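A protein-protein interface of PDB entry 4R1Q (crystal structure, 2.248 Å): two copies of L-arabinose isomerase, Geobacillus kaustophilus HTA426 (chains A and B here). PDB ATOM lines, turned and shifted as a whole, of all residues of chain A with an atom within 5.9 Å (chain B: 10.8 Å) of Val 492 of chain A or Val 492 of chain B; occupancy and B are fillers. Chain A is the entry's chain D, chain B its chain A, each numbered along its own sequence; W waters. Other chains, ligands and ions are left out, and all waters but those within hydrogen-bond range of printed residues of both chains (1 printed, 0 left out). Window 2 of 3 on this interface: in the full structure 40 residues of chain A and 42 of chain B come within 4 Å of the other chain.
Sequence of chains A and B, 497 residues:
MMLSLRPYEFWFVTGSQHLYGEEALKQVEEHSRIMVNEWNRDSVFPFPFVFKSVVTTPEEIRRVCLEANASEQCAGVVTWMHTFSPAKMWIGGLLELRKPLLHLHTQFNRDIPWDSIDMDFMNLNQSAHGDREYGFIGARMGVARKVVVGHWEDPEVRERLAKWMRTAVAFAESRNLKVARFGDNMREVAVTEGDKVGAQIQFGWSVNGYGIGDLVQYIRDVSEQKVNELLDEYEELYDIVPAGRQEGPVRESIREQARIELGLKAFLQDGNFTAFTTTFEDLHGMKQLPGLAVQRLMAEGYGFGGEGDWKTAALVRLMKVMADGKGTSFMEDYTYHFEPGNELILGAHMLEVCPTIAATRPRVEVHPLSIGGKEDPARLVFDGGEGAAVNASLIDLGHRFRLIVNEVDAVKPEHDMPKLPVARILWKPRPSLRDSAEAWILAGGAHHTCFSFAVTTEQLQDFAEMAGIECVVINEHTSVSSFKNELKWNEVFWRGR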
ATOM      1  N   LEU A 487       0.671 -26.808  24.466  1.00  0.00           N
ATOM      2  CA  LEU A 487       0.195 -26.237  23.209  1.00  0.00           C
ATOM      3  C   LEU A 487       1.383 -25.986  22.284  1.00  0.00           C
ATOM      4  O   LEU A 487       1.381 -26.406  21.114  1.00  0.00           O
ATOM      5  CB  LEU A 487      -0.560 -24.927  23.448  1.00  0.00           C
ATOM      6  CG  LEU A 487      -1.916 -24.992  24.159  1.00  0.00           C
ATOM      7  CD1 LEU A 487      -2.446 -23.585  24.387  1.00  0.00           C
ATOM      8  CD2 LEU A 487      -2.912 -25.799  23.336  1.00  0.00           C
ATOM      9  N   LYS A 488       2.397 -25.307  22.822  1.00  0.00           N
ATOM     10  CA  LYS A 488       3.635 -25.030  22.091  1.00  0.00           C
ATOM     11  C   LYS A 488       4.302 -26.282  21.538  1.00  0.00           C
ATOM     12  O   LYS A 488       4.647 -26.337  20.374  1.00  0.00           O
ATOM     13  CB  LYS A 488       4.636 -24.310  22.995  1.00  0.00           C
ATOM     14  CG  LYS A 488       4.328 -22.845  23.236  1.00  0.00           C
ATOM     15  CD  LYS A 488       5.309 -22.252  24.223  1.00  0.00           C
ATOM     16  CE  LYS A 488       5.427 -20.760  24.045  1.00  0.00           C
ATOM     17  NZ  LYS A 488       4.153 -20.083  24.383  1.00  0.00           N
ATOM     18  N   TRP A 489       4.508 -27.288  22.379  1.00  0.00           N
ATOM     19  CA  TRP A 489       5.206 -28.486  21.922  1.00  0.00           C
ATOM     20  C   TRP A 489       4.345 -29.286  20.945  1.00  0.00           C
ATOM     21  O   TRP A 489       4.854 -29.757  19.942  1.00  0.00           O
ATOM     22  CB  TRP A 489       5.689 -29.345  23.092  1.00  0.00           C
ATOM     23  CG  TRP A 489       6.579 -28.592  24.043  1.00  0.00           C
ATOM     24  CD1 TRP A 489       7.479 -27.616  23.727  1.00  0.00           C
ATOM     25  CD2 TRP A 489       6.629 -28.739  25.464  1.00  0.00           C
ATOM     26  NE1 TRP A 489       8.097 -27.156  24.862  1.00  0.00           N
ATOM     27  CE2 TRP A 489       7.592 -27.827  25.945  1.00  0.00           C
ATOM     28  CE3 TRP A 489       5.957 -29.558  26.381  1.00  0.00           C
ATOM     29  CZ2 TRP A 489       7.898 -27.707  27.302  1.00  0.00           C
ATOM     30  CZ3 TRP A 489       6.266 -29.441  27.736  1.00  0.00           C
ATOM     31  CH2 TRP A 489       7.228 -28.522  28.180  1.00  0.00           C
ATOM     32  N   ASN A 490       3.046 -29.407  21.220  1.00  0.00           N
ATOM     33  CA  ASN A 490       2.115 -30.020  20.260  1.00  0.00           C
ATOM     34  C   ASN A 490       2.160 -29.333  18.901  1.00  0.00           C
ATOM     35  O   ASN A 490       2.125 -29.997  17.857  1.00  0.00           O
ATOM     36  CB  ASN A 490       0.671 -29.973  20.765  1.00  0.00           C
ATOM     37  CG  ASN A 490       0.399 -30.958  21.905  1.00  0.00           C
ATOM     38  OD1 ASN A 490       1.280 -31.699  22.342  1.00  0.00           O
ATOM     39  ND2 ASN A 490      -0.833 -30.953  22.392  1.00  0.00           N
ATOM     40  N   GLU A 491       2.229 -27.999  18.919  1.00  0.00           N
ATOM     41  CA  GLU A 491       2.259 -27.225  17.689  1.00  0.00           C
ATOM     42  C   GLU A 491       3.385 -27.682  16.750  1.00  0.00           C
ATOM     43  O   GLU A 491       3.186 -27.781  15.544  1.00  0.00           O
ATOM     44  CB  GLU A 491       2.323 -25.696  17.979  1.00  0.00           C
ATOM     45  CG  GLU A 491       3.725 -25.012  17.998  1.00  0.00           C
ATOM     46  CD  GLU A 491       3.845 -23.840  17.031  1.00  0.00           C
ATOM     47  OE1 GLU A 491       4.795 -23.852  16.196  1.00  0.00           O
ATOM     48  OE2 GLU A 491       3.002 -22.908  17.116  1.00  0.00           O
ATOM     49  N   VAL A 492       4.557 -27.983  17.304  1.00  0.00           N
ATOM     50  CA  VAL A 492       5.676 -28.398  16.464  1.00  0.00           C
ATOM     51  C   VAL A 492       5.489 -29.804  15.913  1.00  0.00           C
ATOM     52  O   VAL A 492       5.773 -30.039  14.754  1.00  0.00           O
ATOM     53  CB  VAL A 492       7.041 -28.289  17.178  1.00  0.00           C
ATOM     54  CG1 VAL A 492       8.127 -28.394  16.155  1.00  0.00           C
ATOM     55  CG2 VAL A 492       7.165 -26.948  17.870  1.00  0.00           C
ATOM     56  N   PHE A 493       4.994 -30.733  16.732  1.00  0.00           N
ATOM     57  CA  PHE A 493       4.686 -32.077  16.239  1.00  0.00           C
ATOM     58  C   PHE A 493       3.594 -32.063  15.160  1.00  0.00           C
ATOM     59  O   PHE A 493       3.726 -32.707  14.125  1.00  0.00           O
ATOM     60  CB  PHE A 493       4.277 -33.000  17.396  1.00  0.00           C
ATOM     61  CG  PHE A 493       3.762 -34.359  16.952  1.00  0.00           C
ATOM     62  CD1 PHE A 493       4.642 -35.397  16.679  1.00  0.00           C
ATOM     63  CD2 PHE A 493       2.396 -34.602  16.829  1.00  0.00           C
ATOM     64  CE1 PHE A 493       4.174 -36.658  16.276  1.00  0.00           C
ATOM     65  CE2 PHE A 493       1.920 -35.849  16.421  1.00  0.00           C
ATOM     66  CZ  PHE A 493       2.815 -36.881  16.147  1.00  0.00           C
ATOM     67  N   TRP A 494       2.511 -31.336  15.394  1.00  0.00           N
ATOM     68  CA  TRP A 494       1.372 -31.391  14.467  1.00  0.00           C
ATOM     69  C   TRP A 494       1.512 -30.625  13.138  1.00  0.00           C
ATOM     70  O   TRP A 494       0.718 -30.835  12.221  1.00  0.00           O
ATOM     71  CB  TRP A 494       0.075 -31.007  15.180  1.00  0.00           C
ATOM     72  CG  TRP A 494      -0.366 -32.074  16.129  1.00  0.00           C
ATOM     73  CD1 TRP A 494      -0.285 -32.050  17.493  1.00  0.00           C
ATOM     74  CD2 TRP A 494      -0.919 -33.345  15.778  1.00  0.00           C
ATOM     75  NE1 TRP A 494      -0.765 -33.227  18.014  1.00  0.00           N
ATOM     76  CE2 TRP A 494      -1.167 -34.037  16.982  1.00  0.00           C
ATOM     77  CE3 TRP A 494      -1.245 -33.959  14.563  1.00  0.00           C
ATOM     78  CZ2 TRP A 494      -1.718 -35.316  17.007  1.00  0.00           C
ATOM     79  CZ3 TRP A 494      -1.791 -35.227  14.590  1.00  0.00           C
ATOM     80  CH2 TRP A 494      -2.018 -35.893  15.805  1.00  0.00           C
ATOM     81  N   ARG A 495       2.508 -29.752  13.016  1.00  0.00           N
ATOM     82  CA  ARG A 495       2.676 -29.008  11.759  1.00  0.00           C
ATOM     83  C   ARG A 495       3.094 -29.912  10.590  1.00  0.00           C
ATOM     84  O   ARG A 495       3.867 -30.851  10.769  1.00  0.00           O
ATOM     85  CB  ARG A 495       3.659 -27.845  11.914  1.00  0.00           C
ATOM     86  CG  ARG A 495       3.550 -26.849  10.759  1.00  0.00           C
ATOM     87  CD  ARG A 495       4.311 -25.541  10.995  1.00  0.00           C
ATOM     88  NE  ARG A 495       3.431 -24.393  11.258  1.00  0.00           N
ATOM     89  CZ  ARG A 495       2.691 -23.779  10.333  1.00  0.00           C
ATOM     90  NH1 ARG A 495       1.931 -22.739  10.665  1.00  0.00           N
ATOM     91  NH2 ARG A 495       2.695 -24.210   9.077  1.00  0.00           N
ATOM     92  N   LEU B 397      22.079 -17.497  22.425  1.00  0.00           N
ATOM     93  CA  LEU B 397      22.400 -18.846  21.974  1.00  0.00           C
ATOM     94  C   LEU B 397      22.917 -18.845  20.536  1.00  0.00           C
ATOM     95  O   LEU B 397      23.157 -19.907  19.947  1.00  0.00           O
ATOM     96  CB  LEU B 397      21.167 -19.727  22.064  1.00  0.00           C
ATOM     97  CG  LEU B 397      20.606 -20.029  23.455  1.00  0.00           C
ATOM     98  CD1 LEU B 397      19.288 -20.799  23.326  1.00  0.00           C
ATOM     99  CD2 LEU B 397      21.615 -20.822  24.242  1.00  0.00           C
ATOM    100  N   HIS B 399      21.367 -18.014  17.622  1.00  0.00           N
ATOM    101  CA  HIS B 399      20.236 -17.785  16.732  1.00  0.00           C
ATOM    102  C   HIS B 399      19.048 -17.134  17.459  1.00  0.00           C
ATOM    103  O   HIS B 399      18.136 -16.613  16.830  1.00  0.00           O
ATOM    104  CB  HIS B 399      19.822 -19.097  16.065  1.00  0.00           C
ATOM    105  CG  HIS B 399      19.435 -20.169  17.035  1.00  0.00           C
ATOM    106  ND1 HIS B 399      20.325 -20.719  17.934  1.00  0.00           N
ATOM    107  CD2 HIS B 399      18.250 -20.793  17.250  1.00  0.00           C
ATOM    108  CE1 HIS B 399      19.705 -21.634  18.662  1.00  0.00           C
ATOM    109  NE2 HIS B 399      18.446 -21.697  18.266  1.00  0.00           N
ATOM    110  N   ARG B 400      19.068 -17.151  18.786  1.00  0.00           N
ATOM    111  CA  ARG B 400      18.009 -16.517  19.552  1.00  0.00           C
ATOM    112  C   ARG B 400      18.508 -16.256  20.959  1.00  0.00           C
ATOM    113  O   ARG B 400      19.588 -16.713  21.328  1.00  0.00           O
ATOM    114  CB  ARG B 400      16.756 -17.404  19.598  1.00  0.00           C
ATOM    115  CG  ARG B 400      16.995 -18.758  20.262  1.00  0.00           C
ATOM    116  CD  ARG B 400      15.808 -19.669  20.087  1.00  0.00           C
ATOM    117  NE  ARG B 400      16.011 -20.943  20.767  1.00  0.00           N
ATOM    118  CZ  ARG B 400      15.738 -21.161  22.052  1.00  0.00           C
ATOM    119  NH1 ARG B 400      15.250 -20.191  22.813  1.00  0.00           N
ATOM    120  NH2 ARG B 400      15.976 -22.352  22.587  1.00  0.00           N
ATOM    121  N   ARG B 402      17.707 -16.256  25.297  1.00  0.00           N
ATOM    122  CA  ARG B 402      17.042 -17.082  26.300  1.00  0.00           C
ATOM    123  C   ARG B 402      17.177 -16.398  27.641  1.00  0.00           C
ATOM    124  O   ARG B 402      18.270 -16.026  28.030  1.00  0.00           O
ATOM    125  CB  ARG B 402      17.704 -18.467  26.389  1.00  0.00           C
ATOM    126  CG  ARG B 402      17.146 -19.311  27.548  1.00  0.00           C
ATOM    127  CD  ARG B 402      17.906 -20.603  27.752  1.00  0.00           C
ATOM    128  NE  ARG B 402      17.646 -21.573  26.695  1.00  0.00           N
ATOM    129  CZ  ARG B 402      18.477 -22.557  26.370  1.00  0.00           C
ATOM    130  NH1 ARG B 402      19.636 -22.698  27.011  1.00  0.00           N
ATOM    131  NH2 ARG B 402      18.147 -23.403  25.401  1.00  0.00           N
ATOM    132  N   GLU B 470      12.207 -17.216  24.669  1.00  0.00           N
ATOM    133  CA  GLU B 470      12.107 -18.269  25.672  1.00  0.00           C
ATOM    134  C   GLU B 470      12.474 -17.780  27.067  1.00  0.00           C
ATOM    135  O   GLU B 470      13.448 -17.071  27.246  1.00  0.00           O
ATOM    136  CB  GLU B 470      13.028 -19.433  25.299  1.00  0.00           C
ATOM    137  CG  GLU B 470      13.014 -20.596  26.278  1.00  0.00           C
ATOM    138  CD  GLU B 470      14.130 -21.620  26.020  1.00  0.00           C
ATOM    139  OE1 GLU B 470      15.123 -21.322  25.305  1.00  0.00           O
ATOM    140  OE2 GLU B 470      14.001 -22.745  26.531  1.00  0.00           O
ATOM    141  N   LYS B 484      15.691 -30.581  31.680  1.00  0.00           N
ATOM    142  CA  LYS B 484      16.480 -30.987  30.531  1.00  0.00           C
ATOM    143  C   LYS B 484      15.560 -31.227  29.334  1.00  0.00           C
ATOM    144  O   LYS B 484      15.866 -30.825  28.218  1.00  0.00           O
ATOM    145  CB  LYS B 484      17.252 -32.258  30.872  1.00  0.00           C
ATOM    146  CG  LYS B 484      18.683 -32.295  30.390  1.00  0.00           C
ATOM    147  CD  LYS B 484      19.370 -33.582  30.861  1.00  0.00           C
ATOM    148  CE  LYS B 484      20.684 -33.814  30.122  1.00  0.00           C
ATOM    149  NZ  LYS B 484      20.532 -33.688  28.641  1.00  0.00           N
ATOM    150  N   ASN B 485      14.429 -31.879  29.574  1.00  0.00           N
ATOM    151  CA  ASN B 485      13.461 -32.119  28.510  1.00  0.00           C
ATOM    152  C   ASN B 485      12.854 -30.834  27.980  1.00  0.00           C
ATOM    153  O   ASN B 485      12.687 -30.673  26.775  1.00  0.00           O
ATOM    154  CB  ASN B 485      12.337 -33.037  28.982  1.00  0.00           C
ATOM    155  CG  ASN B 485      12.762 -34.491  29.059  1.00  0.00           C
ATOM    156  OD1 ASN B 485      13.753 -34.897  28.445  1.00  0.00           O
ATOM    157  ND2 ASN B 485      12.002 -35.289  29.807  1.00  0.00           N
ATOM    158  N   GLU B 486      12.506 -29.926  28.884  1.00  0.00           N
ATOM    159  CA  GLU B 486      11.870 -28.684  28.465  1.00  0.00           C
ATOM    160  C   GLU B 486      12.788 -27.818  27.608  1.00  0.00           C
ATOM    161  O   GLU B 486      12.324 -27.189  26.670  1.00  0.00           O
ATOM    162  CB  GLU B 486      11.339 -27.911  29.657  1.00  0.00           C
ATOM    163  CG  GLU B 486      10.245 -28.655  30.393  1.00  0.00           C
ATOM    164  CD  GLU B 486       9.695 -27.865  31.562  1.00  0.00           C
ATOM    165  OE1 GLU B 486      10.098 -26.681  31.730  1.00  0.00           O
ATOM    166  OE2 GLU B 486       8.869 -28.438  32.307  1.00  0.00           O
ATOM    167  N   LEU B 487      14.080 -27.808  27.911  1.00  0.00           N
ATOM    168  CA  LEU B 487      15.056 -27.135  27.053  1.00  0.00           C
ATOM    169  C   LEU B 487      15.046 -27.709  25.635  1.00  0.00           C
ATOM    170  O   LEU B 487      15.117 -26.966  24.649  1.00  0.00           O
ATOM    171  CB  LEU B 487      16.467 -27.268  27.634  1.00  0.00           C
ATOM    172  CG  LEU B 487      16.798 -26.530  28.933  1.00  0.00           C
ATOM    173  CD1 LEU B 487      18.239 -26.822  29.379  1.00  0.00           C
ATOM    174  CD2 LEU B 487      16.576 -25.033  28.767  1.00  0.00           C
ATOM    175  N   LYS B 488      14.996 -29.033  25.536  1.00  0.00           N
ATOM    176  CA  LYS B 488      14.929 -29.704  24.232  1.00  0.00           C
ATOM    177  C   LYS B 488      13.661 -29.320  23.461  1.00  0.00           C
ATOM    178  O   LYS B 488      13.727 -28.859  22.329  1.00  0.00           O
ATOM    179  CB  LYS B 488      14.997 -31.232  24.406  1.00  0.00           C
ATOM    180  CG  LYS B 488      16.414 -31.794  24.624  1.00  0.00           C
ATOM    181  CD  LYS B 488      16.342 -33.196  25.196  1.00  0.00           C
ATOM    182  CE  LYS B 488      17.612 -34.007  24.915  1.00  0.00           C
ATOM    183  NZ  LYS B 488      18.813 -33.448  25.585  1.00  0.00           N
ATOM    184  N   TRP B 489      12.506 -29.509  24.080  1.00  0.00           N
ATOM    185  CA  TRP B 489      11.241 -29.264  23.395  1.00  0.00           C
ATOM    186  C   TRP B 489      11.072 -27.765  23.097  1.00  0.00           C
ATOM    187  O   TRP B 489      10.630 -27.381  22.013  1.00  0.00           O
ATOM    188  CB  TRP B 489      10.085 -29.811  24.227  1.00  0.00           C
ATOM    189  CG  TRP B 489      10.227 -31.275  24.557  1.00  0.00           C
ATOM    190  CD1 TRP B 489      10.834 -32.235  23.795  1.00  0.00           C
ATOM    191  CD2 TRP B 489       9.759 -31.936  25.733  1.00  0.00           C
ATOM    192  NE1 TRP B 489      10.768 -33.452  24.425  1.00  0.00           N
ATOM    193  CE2 TRP B 489      10.118 -33.296  25.620  1.00  0.00           C
ATOM    194  CE3 TRP B 489       9.066 -31.510  26.877  1.00  0.00           C
ATOM    195  CZ2 TRP B 489       9.802 -34.236  26.599  1.00  0.00           C
ATOM    196  CZ3 TRP B 489       8.765 -32.437  27.853  1.00  0.00           C
ATOM    197  CH2 TRP B 489       9.124 -33.793  27.704  1.00  0.00           C
ATOM    198  N   ASN B 490      11.453 -26.925  24.049  1.00  0.00           N
ATOM    199  CA  ASN B 490      11.513 -25.490  23.798  1.00  0.00           C
ATOM    200  C   ASN B 490      12.362 -25.122  22.594  1.00  0.00           C
ATOM    201  O   ASN B 490      11.998 -24.234  21.837  1.00  0.00           O
ATOM    202  CB  ASN B 490      12.019 -24.743  25.026  1.00  0.00           C
ATOM    203  CG  ASN B 490      10.935 -24.540  26.071  1.00  0.00           C
ATOM    204  OD1 ASN B 490       9.821 -25.053  25.935  1.00  0.00           O
ATOM    205  ND2 ASN B 490      11.258 -23.785  27.116  1.00  0.00           N
ATOM    206  N   GLU B 491      13.490 -25.809  22.421  1.00  0.00           N
ATOM    207  CA  GLU B 491      14.414 -25.542  21.313  1.00  0.00           C
ATOM    208  C   GLU B 491      13.743 -25.655  19.946  1.00  0.00           C
ATOM    209  O   GLU B 491      13.930 -24.805  19.071  1.00  0.00           O
ATOM    210  CB  GLU B 491      15.685 -26.450  21.408  1.00  0.00           C
ATOM    211  CG  GLU B 491      15.814 -27.693  20.460  1.00  0.00           C
ATOM    212  CD  GLU B 491      16.345 -27.376  19.022  1.00  0.00           C
ATOM    213  OE1 GLU B 491      16.885 -26.260  18.779  1.00  0.00           O
ATOM    214  OE2 GLU B 491      16.231 -28.263  18.132  1.00  0.00           O
ATOM    215  N   VAL B 492      12.942 -26.694  19.772  1.00  0.00           N
ATOM    216  CA  VAL B 492      12.333 -26.936  18.488  1.00  0.00           C
ATOM    217  C   VAL B 492      11.254 -25.892  18.225  1.00  0.00           C
ATOM    218  O   VAL B 492      11.049 -25.481  17.089  1.00  0.00           O
ATOM    219  CB  VAL B 492      11.740 -28.346  18.402  1.00  0.00           C
ATOM    220  CG1 VAL B 492      11.469 -28.673  16.967  1.00  0.00           C
ATOM    221  CG2 VAL B 492      12.715 -29.358  18.953  1.00  0.00           C
ATOM    222  N   PHE B 493      10.575 -25.451  19.278  1.00  0.00           N
ATOM    223  CA  PHE B 493       9.536 -24.442  19.116  1.00  0.00           C
ATOM    224  C   PHE B 493      10.110 -23.067  18.774  1.00  0.00           C
ATOM    225  O   PHE B 493       9.607 -22.386  17.891  1.00  0.00           O
ATOM    226  CB  PHE B 493       8.652 -24.337  20.364  1.00  0.00           C
ATOM    227  CG  PHE B 493       7.689 -23.186  20.308  1.00  0.00           C
ATOM    228  CD1 PHE B 493       6.519 -23.280  19.564  1.00  0.00           C
ATOM    229  CD2 PHE B 493       7.962 -21.992  20.975  1.00  0.00           C
ATOM    230  CE1 PHE B 493       5.625 -22.205  19.494  1.00  0.00           C
ATOM    231  CE2 PHE B 493       7.076 -20.915  20.912  1.00  0.00           C
ATOM    232  CZ  PHE B 493       5.902 -21.026  20.164  1.00  0.00           C
ATOM    233  N   TRP B 494      11.150 -22.657  19.489  1.00  0.00           N
ATOM    234  CA  TRP B 494      11.684 -21.315  19.330  1.00  0.00           C
ATOM    235  C   TRP B 494      12.634 -21.175  18.134  1.00  0.00           C
ATOM    236  O   TRP B 494      13.036 -20.074  17.782  1.00  0.00           O
ATOM    237  CB  TRP B 494      12.360 -20.849  20.619  1.00  0.00           C
ATOM    238  CG  TRP B 494      11.385 -20.535  21.726  1.00  0.00           C
ATOM    239  CD1 TRP B 494      11.128 -21.290  22.833  1.00  0.00           C
ATOM    240  CD2 TRP B 494      10.526 -19.389  21.814  1.00  0.00           C
ATOM    241  NE1 TRP B 494      10.172 -20.687  23.606  1.00  0.00           N
ATOM    242  CE2 TRP B 494       9.790 -19.512  23.010  1.00  0.00           C
ATOM    243  CE3 TRP B 494      10.322 -18.258  21.003  1.00  0.00           C
ATOM    244  CZ2 TRP B 494       8.845 -18.557  23.416  1.00  0.00           C
ATOM    245  CZ3 TRP B 494       9.384 -17.310  21.406  1.00  0.00           C
ATOM    246  CH2 TRP B 494       8.659 -17.471  22.606  1.00  0.00           C
ATOM    247  N   ARG B 495      12.982 -22.291  17.506  1.00  0.00           N
ATOM    248  CA  ARG B 495      13.808 -22.267  16.294  1.00  0.00           C
ATOM    249  C   ARG B 495      13.091 -21.547  15.139  1.00  0.00           C
ATOM    250  O   ARG B 495      11.967 -21.911  14.769  1.00  0.00           O
ATOM    251  CB  ARG B 495      14.167 -23.697  15.868  1.00  0.00           C
ATOM    252  CG  ARG B 495      15.241 -23.784  14.784  1.00  0.00           C
ATOM    253  CD  ARG B 495      16.635 -24.021  15.383  1.00  0.00           C
ATOM    254  NE  ARG B 495      17.693 -23.430  14.561  1.00  0.00           N
ATOM    255  CZ  ARG B 495      18.998 -23.627  14.750  1.00  0.00           C
ATOM    256  NH1 ARG B 495      19.877 -23.036  13.950  1.00  0.00           N
ATOM    257  NH2 ARG B 495      19.427 -24.414  15.731  1.00  0.00           N
ATOM    258  N   GLY B 496      13.742 -20.527  14.582  1.00  0.00           N
ATOM    259  CA  GLY B 496      13.250 -19.840  13.396  1.00  0.00           C
ATOM    260  C   GLY B 496      11.887 -19.182  13.555  1.00  0.00           C
ATOM    261  O   GLY B 496      11.293 -18.713  12.575  1.00  0.00           O
HETATM  262  O   HOH W   1       7.627 -22.980  15.879  1.00  0.00           O
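The side-chain amide oxygen (OD1) of Asn 490 of chain B sits at hydrogen-bond distance from the indole nitrogen (NE1) of Trp 489 of chain A.
O of Glu 486 of chain B sits close to OD1 of Asn 490 of chain B (3.4 Å). OE2 of Glu 470 of chain B lies within hydrogen-bond range of ND2 of Asn 490 of chain B.
Lys 488 of chain A touches Phe 493 of chain B (CE to CE2, 3.5 Å). Glu 486 of chain B touches Trp 489 of chain A (CG to CH2, 3.7 Å). CB of Trp 489 of chain B touches NE1 of Trp 489 of chain A (3.4 Å). Glu 491 of chain A touches Phe 493 of chain B. Val 492 of chain B touches Val 492 of chain A (CG1 to CG1, 3.5 Å). Val 492 of chain A touches Phe 493 of chain B.
Of chain B, only Val 492 (3.5 Å) and Phe 493 (3.7 Å) come within 4 Å of Val 492 of chain A. Of the printed residues of chain A, Val 492 of chain B touches Val 492 (3.5 Å). Of the printed residues of chain A, Phe 493 of chain B touches Lys 488 (3.5 Å), Glu 491 (3.5 Å) and Val 492 (3.7 Å). Of the printed residues of chain B, Lys 488 of chain A touches Phe 493. Printed residues of chain A within 4 Å of Asn 490 of chain B: Trp 489 (2.9 Å). Asn 490 of chain A touches none of the printed residues of chain B. Leu 487 of chain B touches none of the printed residues of chain A. The nearest residue of chain B that does not touch Val 492 of chain A is Trp 489 of chain B (5.4 Å). The nearest printed residue of chain A that does not touch Val 492 of chain B is Glu 491 of chain A (6.5 Å). The nearest printed residue of chain A that does not touch Phe 493 of chain B is Trp 489 of chain A (4.8 Å).
Of the 9 printed residues of chain A, 4 touch a printed residue of chain B. Hydrophobic or aromatic side chains of chain A within 4 Å of the printed part of chain B: Trp 489 and Val 492. Of the 18 printed residues of chain B, 5 touch a printed residue of chain A. Among the printed residues, 7 pairs touch across the chains.
Trp 489 of chain A touches its own counterpart, Trp 489 of chain B. Glu 491 of chain A touches Phe 493 of chain B, but with the chains exchanged Phe 493 of chain A does not touch Glu 491 of chain B (10.6 Å). Val 492 of chain B touches its own counterpart, Val 492 of chain A. Val 492 of chain A touches Phe 493 of chain B, but with the chains exchanged Phe 493 of chain A does not touch Val 492 of chain B (6.8 Å). 9 positions are printed for both chains.
Water W1 lies within hydrogen-bond range of the backbone carbonyl oxygen (O) of Phe 493 of chain B and the side-chain carboxylate (OE1) of Glu 491 of chain A.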
